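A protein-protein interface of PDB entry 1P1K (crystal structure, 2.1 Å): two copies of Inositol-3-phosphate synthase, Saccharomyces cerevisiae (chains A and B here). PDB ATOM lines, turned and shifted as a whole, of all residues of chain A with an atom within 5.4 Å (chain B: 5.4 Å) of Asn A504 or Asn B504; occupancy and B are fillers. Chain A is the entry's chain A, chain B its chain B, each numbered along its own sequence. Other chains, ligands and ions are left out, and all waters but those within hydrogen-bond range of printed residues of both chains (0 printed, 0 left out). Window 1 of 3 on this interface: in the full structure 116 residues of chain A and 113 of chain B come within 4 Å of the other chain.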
ATOM      1  N   VAL A 331     -11.549  -5.362 -17.959  1.00  0.00           N
ATOM      2  CA  VAL A 331     -11.863  -5.106 -19.357  1.00  0.00           C
ATOM      3  C   VAL A 331     -11.970  -3.600 -19.628  1.00  0.00           C
ATOM      4  O   VAL A 331     -11.455  -3.099 -20.629  1.00  0.00           O
ATOM      5  CB  VAL A 331     -13.196  -5.795 -19.758  1.00  0.00           C
ATOM      6  CG1 VAL A 331     -13.576  -5.436 -21.184  1.00  0.00           C
ATOM      7  CG2 VAL A 331     -13.061  -7.301 -19.622  1.00  0.00           C
ATOM      8  N   GLN A 334      -8.457  -1.574 -18.867  1.00  0.00           N
ATOM      9  CA  GLN A 334      -7.540  -1.896 -19.947  1.00  0.00           C
ATOM     10  C   GLN A 334      -7.927  -1.021 -21.125  1.00  0.00           C
ATOM     11  O   GLN A 334      -7.112  -0.285 -21.665  1.00  0.00           O
ATOM     12  CB  GLN A 334      -7.695  -3.365 -20.340  1.00  0.00           C
ATOM     13  CG  GLN A 334      -6.659  -3.859 -21.318  1.00  0.00           C
ATOM     14  CD  GLN A 334      -5.264  -3.862 -20.729  1.00  0.00           C
ATOM     15  OE1 GLN A 334      -4.669  -2.806 -20.493  1.00  0.00           O
ATOM     16  NE2 GLN A 334      -4.738  -5.055 -20.474  1.00  0.00           N
ATOM     17  N   PHE A 335      -9.190  -1.115 -21.510  1.00  0.00           N
ATOM     18  CA  PHE A 335      -9.726  -0.344 -22.611  1.00  0.00           C
ATOM     19  C   PHE A 335      -9.349   1.138 -22.524  1.00  0.00           C
ATOM     20  O   PHE A 335      -8.883   1.723 -23.502  1.00  0.00           O
ATOM     21  CB  PHE A 335     -11.252  -0.490 -22.641  1.00  0.00           C
ATOM     22  CG  PHE A 335     -11.949   0.577 -23.436  1.00  0.00           C
ATOM     23  CD1 PHE A 335     -11.872   0.599 -24.819  1.00  0.00           C
ATOM     24  CD2 PHE A 335     -12.645   1.591 -22.793  1.00  0.00           C
ATOM     25  CE1 PHE A 335     -12.478   1.618 -25.548  1.00  0.00           C
ATOM     26  CE2 PHE A 335     -13.248   2.605 -23.510  1.00  0.00           C
ATOM     27  CZ  PHE A 335     -13.163   2.620 -24.892  1.00  0.00           C
ATOM     28  N   GLY A 502      -4.956  -8.760 -17.656  1.00  0.00           N
ATOM     29  CA  GLY A 502      -5.683  -8.382 -18.858  1.00  0.00           C
ATOM     30  C   GLY A 502      -6.602  -9.495 -19.314  1.00  0.00           C
ATOM     31  O   GLY A 502      -6.160 -10.454 -19.954  1.00  0.00           O
ATOM     32  N   LEU A 503      -7.884  -9.364 -18.994  1.00  0.00           N
ATOM     33  CA  LEU A 503      -8.858 -10.388 -19.342  1.00  0.00           C
ATOM     34  C   LEU A 503      -8.846 -10.839 -20.797  1.00  0.00           C
ATOM     35  O   LEU A 503      -8.821 -12.037 -21.080  1.00  0.00           O
ATOM     36  CB  LEU A 503     -10.274  -9.933 -18.989  1.00  0.00           C
ATOM     37  CG  LEU A 503     -11.286 -11.084 -18.988  1.00  0.00           C
ATOM     38  CD1 LEU A 503     -11.064 -11.951 -17.741  1.00  0.00           C
ATOM     39  CD2 LEU A 503     -12.703 -10.530 -18.993  1.00  0.00           C
ATOM     40  N   ASN A 504      -8.875  -9.887 -21.722  1.00  0.00           N
ATOM     41  CA  ASN A 504      -8.902 -10.225 -23.141  1.00  0.00           C
ATOM     42  C   ASN A 504      -7.654 -10.964 -23.566  1.00  0.00           C
ATOM     43  O   ASN A 504      -7.710 -11.833 -24.436  1.00  0.00           O
ATOM     44  CB  ASN A 504      -9.101  -8.961 -23.974  1.00  0.00           C
ATOM     45  CG  ASN A 504     -10.456  -8.321 -23.727  1.00  0.00           C
ATOM     46  OD1 ASN A 504     -11.497  -8.904 -24.045  1.00  0.00           O
ATOM     47  ND2 ASN A 504     -10.452  -7.127 -23.142  1.00  0.00           N
ATOM     48  N   LYS A 505      -6.530 -10.620 -22.942  1.00  0.00           N
ATOM     49  CA  LYS A 505      -5.266 -11.279 -23.236  1.00  0.00           C
ATOM     50  C   LYS A 505      -5.265 -12.678 -22.616  1.00  0.00           C
ATOM     51  O   LYS A 505      -4.700 -13.620 -23.188  1.00  0.00           O
ATOM     52  CB  LYS A 505      -4.105 -10.456 -22.687  1.00  0.00           C
ATOM     53  CG  LYS A 505      -3.952  -9.124 -23.381  1.00  0.00           C
ATOM     54  CD  LYS A 505      -2.694  -8.392 -22.952  1.00  0.00           C
ATOM     55  CE  LYS A 505      -2.787  -7.880 -21.525  1.00  0.00           C
ATOM     56  NZ  LYS A 505      -1.593  -7.057 -21.186  1.00  0.00           N
ATOM     57  N   GLN A 506      -5.910 -12.813 -21.452  1.00  0.00           N
ATOM     58  CA  GLN A 506      -5.990 -14.103 -20.771  1.00  0.00           C
ATOM     59  C   GLN A 506      -6.800 -15.078 -21.615  1.00  0.00           C
ATOM     60  O   GLN A 506      -6.467 -16.258 -21.677  1.00  0.00           O
ATOM     61  CB  GLN A 506      -6.618 -13.954 -19.373  1.00  0.00           C
ATOM     62  CG  GLN A 506      -5.875 -12.967 -18.463  1.00  0.00           C
ATOM     63  CD  GLN A 506      -6.493 -12.812 -17.072  1.00  0.00           C
ATOM     64  OE1 GLN A 506      -7.714 -12.713 -16.917  1.00  0.00           O
ATOM     65  NE2 GLN A 506      -5.640 -12.771 -16.054  1.00  0.00           N
ATOM     66  N   ARG A 507      -7.852 -14.602 -22.277  1.00  0.00           N
ATOM     67  CA  ARG A 507      -8.648 -15.512 -23.101  1.00  0.00           C
ATOM     68  C   ARG A 507      -7.919 -15.805 -24.407  1.00  0.00           C
ATOM     69  O   ARG A 507      -7.994 -16.922 -24.929  1.00  0.00           O
ATOM     70  CB  ARG A 507     -10.044 -14.945 -23.413  1.00  0.00           C
ATOM     71  CG  ARG A 507     -10.947 -15.951 -24.165  1.00  0.00           C
ATOM     72  CD  ARG A 507     -12.363 -15.432 -24.398  1.00  0.00           C
ATOM     73  NE  ARG A 507     -13.282 -16.477 -24.871  1.00  0.00           N
ATOM     74  CZ  ARG A 507     -13.712 -16.609 -26.128  1.00  0.00           C
ATOM     75  NH1 ARG A 507     -14.549 -17.589 -26.449  1.00  0.00           N
ATOM     76  NH2 ARG A 507     -13.310 -15.767 -27.073  1.00  0.00           N
ATOM     77  N   THR A 508      -7.215 -14.799 -24.924  1.00  0.00           N
ATOM     78  CA  THR A 508      -6.459 -14.947 -26.164  1.00  0.00           C
ATOM     79  C   THR A 508      -5.438 -16.068 -25.996  1.00  0.00           C
ATOM     80  O   THR A 508      -5.296 -16.918 -26.879  1.00  0.00           O
ATOM     81  CB  THR A 508      -5.733 -13.634 -26.543  1.00  0.00           C
ATOM     82  OG1 THR A 508      -6.706 -12.624 -26.848  1.00  0.00           O
ATOM     83  CG2 THR A 508      -4.836 -13.846 -27.755  1.00  0.00           C
ATOM     84  N   ALA A 509      -4.739 -16.076 -24.859  1.00  0.00           N
ATOM     85  CA  ALA A 509      -3.749 -17.118 -24.569  1.00  0.00           C
ATOM     86  C   ALA A 509      -4.418 -18.479 -24.674  1.00  0.00           C
ATOM     87  O   ALA A 509      -3.894 -19.391 -25.305  1.00  0.00           O
ATOM     88  CB  ALA A 509      -3.177 -16.929 -23.171  1.00  0.00           C
ATOM     89  N   VAL B 331     -17.309  -3.078 -26.737  1.00  0.00           N
ATOM     90  CA  VAL B 331     -16.347  -3.877 -25.990  1.00  0.00           C
ATOM     91  C   VAL B 331     -17.033  -4.722 -24.908  1.00  0.00           C
ATOM     92  O   VAL B 331     -16.796  -5.925 -24.817  1.00  0.00           O
ATOM     93  CB  VAL B 331     -15.253  -2.981 -25.361  1.00  0.00           C
ATOM     94  CG1 VAL B 331     -14.429  -3.767 -24.349  1.00  0.00           C
ATOM     95  CG2 VAL B 331     -14.340  -2.468 -26.456  1.00  0.00           C
ATOM     96  N   ASP B 338     -18.201 -13.384 -25.033  1.00  0.00           N
ATOM     97  CA  ASP B 338     -16.982 -14.190 -24.974  1.00  0.00           C
ATOM     98  C   ASP B 338     -16.997 -15.016 -23.697  1.00  0.00           C
ATOM     99  O   ASP B 338     -16.304 -16.029 -23.586  1.00  0.00           O
ATOM    100  CB  ASP B 338     -15.739 -13.299 -24.963  1.00  0.00           C
ATOM    101  CG  ASP B 338     -15.394 -12.757 -26.333  1.00  0.00           C
ATOM    102  OD1 ASP B 338     -14.640 -11.766 -26.384  1.00  0.00           O
ATOM    103  OD2 ASP B 338     -15.863 -13.321 -27.350  1.00  0.00           O
ATOM    104  N   GLY B 502     -15.202  -5.163 -33.522  1.00  0.00           N
ATOM    105  CA  GLY B 502     -14.561  -5.539 -32.270  1.00  0.00           C
ATOM    106  C   GLY B 502     -13.387  -4.610 -32.069  1.00  0.00           C
ATOM    107  O   GLY B 502     -12.358  -4.753 -32.723  1.00  0.00           O
ATOM    108  N   LEU B 503     -13.550  -3.648 -31.169  1.00  0.00           N
ATOM    109  CA  LEU B 503     -12.521  -2.651 -30.902  1.00  0.00           C
ATOM    110  C   LEU B 503     -11.140  -3.194 -30.536  1.00  0.00           C
ATOM    111  O   LEU B 503     -10.120  -2.665 -30.989  1.00  0.00           O
ATOM    112  CB  LEU B 503     -12.991  -1.701 -29.800  1.00  0.00           C
ATOM    113  CG  LEU B 503     -12.199  -0.395 -29.712  1.00  0.00           C
ATOM    114  CD1 LEU B 503     -12.697   0.609 -30.755  1.00  0.00           C
ATOM    115  CD2 LEU B 503     -12.348   0.168 -28.320  1.00  0.00           C
ATOM    116  N   ASN B 504     -11.097  -4.232 -29.707  1.00  0.00           N
ATOM    117  CA  ASN B 504      -9.815  -4.802 -29.309  1.00  0.00           C
ATOM    118  C   ASN B 504      -9.125  -5.412 -30.510  1.00  0.00           C
ATOM    119  O   ASN B 504      -7.900  -5.400 -30.603  1.00  0.00           O
ATOM    120  CB  ASN B 504      -9.996  -5.864 -28.218  1.00  0.00           C
ATOM    121  CG  ASN B 504     -10.269  -5.255 -26.848  1.00  0.00           C
ATOM    122  OD1 ASN B 504     -10.160  -5.934 -25.826  1.00  0.00           O
ATOM    123  ND2 ASN B 504     -10.629  -3.972 -26.822  1.00  0.00           N
ATOM    124  N   LYS B 505      -9.923  -5.941 -31.431  1.00  0.00           N
ATOM    125  CA  LYS B 505      -9.399  -6.555 -32.643  1.00  0.00           C
ATOM    126  C   LYS B 505      -8.995  -5.489 -33.672  1.00  0.00           C
ATOM    127  O   LYS B 505      -8.137  -5.728 -34.526  1.00  0.00           O
ATOM    128  CB  LYS B 505     -10.447  -7.498 -33.231  1.00  0.00           C
ATOM    129  CG  LYS B 505     -10.912  -8.570 -32.255  1.00  0.00           C
ATOM    130  CD  LYS B 505     -11.999  -9.441 -32.864  1.00  0.00           C
ATOM    131  CE  LYS B 505     -13.208  -8.614 -33.277  1.00  0.00           C
ATOM    132  NZ  LYS B 505     -14.275  -9.456 -33.882  1.00  0.00           N
ATOM    133  N   GLN B 506      -9.617  -4.315 -33.588  1.00  0.00           N
ATOM    134  CA  GLN B 506      -9.308  -3.215 -34.491  1.00  0.00           C
ATOM    135  C   GLN B 506      -7.990  -2.584 -34.061  1.00  0.00           C
ATOM    136  O   GLN B 506      -7.304  -1.946 -34.861  1.00  0.00           O
ATOM    137  CB  GLN B 506     -10.437  -2.180 -34.473  1.00  0.00           C
ATOM    138  CG  GLN B 506     -11.691  -2.651 -35.210  1.00  0.00           C
ATOM    139  CD  GLN B 506     -12.907  -1.764 -34.990  1.00  0.00           C
ATOM    140  OE1 GLN B 506     -13.867  -1.818 -35.762  1.00  0.00           O
ATOM    141  NE2 GLN B 506     -12.883  -0.959 -33.931  1.00  0.00           N
ATOM    142  N   ARG B 507      -7.637  -2.767 -32.790  1.00  0.00           N
ATOM    143  CA  ARG B 507      -6.384  -2.234 -32.276  1.00  0.00           C
ATOM    144  C   ARG B 507      -5.329  -3.327 -32.356  1.00  0.00           C
ATOM    145  O   ARG B 507      -4.138  -3.044 -32.415  1.00  0.00           O
ATOM    146  CB  ARG B 507      -6.534  -1.762 -30.831  1.00  0.00           C
ATOM    147  CG  ARG B 507      -5.250  -1.191 -30.258  1.00  0.00           C
ATOM    148  CD  ARG B 507      -5.486  -0.560 -28.914  1.00  0.00           C
ATOM    149  NE  ARG B 507      -4.340   0.214 -28.433  1.00  0.00           N
ATOM    150  CZ  ARG B 507      -3.263  -0.310 -27.849  1.00  0.00           C
ATOM    151  NH1 ARG B 507      -2.282   0.488 -27.447  1.00  0.00           N
ATOM    152  NH2 ARG B 507      -3.166  -1.625 -27.658  1.00  0.00           N
ATOM    153  N   THR B 508      -5.775  -4.579 -32.350  1.00  0.00           N
ATOM    154  CA  THR B 508      -4.858  -5.707 -32.448  1.00  0.00           C
ATOM    155  C   THR B 508      -4.332  -5.749 -33.875  1.00  0.00           C
ATOM    156  O   THR B 508      -3.203  -6.153 -34.116  1.00  0.00           O
ATOM    157  CB  THR B 508      -5.555  -7.053 -32.100  1.00  0.00           C
ATOM    158  OG1 THR B 508      -5.769  -7.122 -30.688  1.00  0.00           O
ATOM    159  CG2 THR B 508      -4.699  -8.238 -32.520  1.00  0.00           C
ATOM    160  N   ALA B 509      -5.161  -5.318 -34.816  1.00  0.00           N
ATOM    161  CA  ALA B 509      -4.768  -5.286 -36.215  1.00  0.00           C
ATOM    162  C   ALA B 509      -3.652  -4.256 -36.366  1.00  0.00           C
ATOM    163  O   ALA B 509      -2.565  -4.567 -36.842  1.00  0.00           O
ATOM    164  CB  ALA B 509      -5.961  -4.903 -37.080  1.00  0.00           C
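The backbone carbonyl oxygen (O) of Asn A504 sits at hydrogen-bond distance from the side-chain hydroxyl (OG1) of Thr A508 (2.7 Å).
The backbone carbonyl oxygen of Asn B504 is in hydrogen-bond range of the side-chain hydroxyl of Thr B508, 2.7 Å away.
Val A331 touches its own counterpart, Val B331.
Asn B504 touches its own counterpart, Asn A504.
Positions printed for both chains: 331, 502, 503, 504, 505, 506, 507, 508 and 509.
Among the printed residues, 4 pairs touch across the chains.
Among the printed residues, Asp or Glu carboxylates within 4 Å of a Lys or Arg side-chain nitrogen of the other chain: Arg A507 with Asp B338.
Printed residues of chain B within 4 Å of Val A331: Val B331 (3.7 Å).
Of chain B, only Asn B504 (3.0 Å) comes within 4 Å of Asn A504.
Printed residues of chain A within 4 Å of Asp B338: Arg A507.
Of the printed residues of chain A, Leu B503 touches Phe A335 (3.1 Å).
Asn B504 touches just one residue of chain A: Asn A504 (3.0 Å).
Arg B507 touches none of the printed residues of chain A.
The nearest residue of chain B that does not touch Asn A504 is Asp B338 (4.9 Å).
The nearest residue of chain A that does not touch Asn B504 is Phe A335 (5.1 Å).
The nearest printed residue of chain B that does not touch Phe A335 is Val B331 (4.3 Å).
CG1 of Val A331 touches CG1 of Val B331 (3.7 Å).
Phe A335 touches Leu B503.
OD1 of Asn B504 sits at hydrogen-bond distance from ND2 of Asn A504 (3.0 Å).
NH2 of Arg A507 is in salt-bridge range of OD2 of Asp B338, at 3.5 Å.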
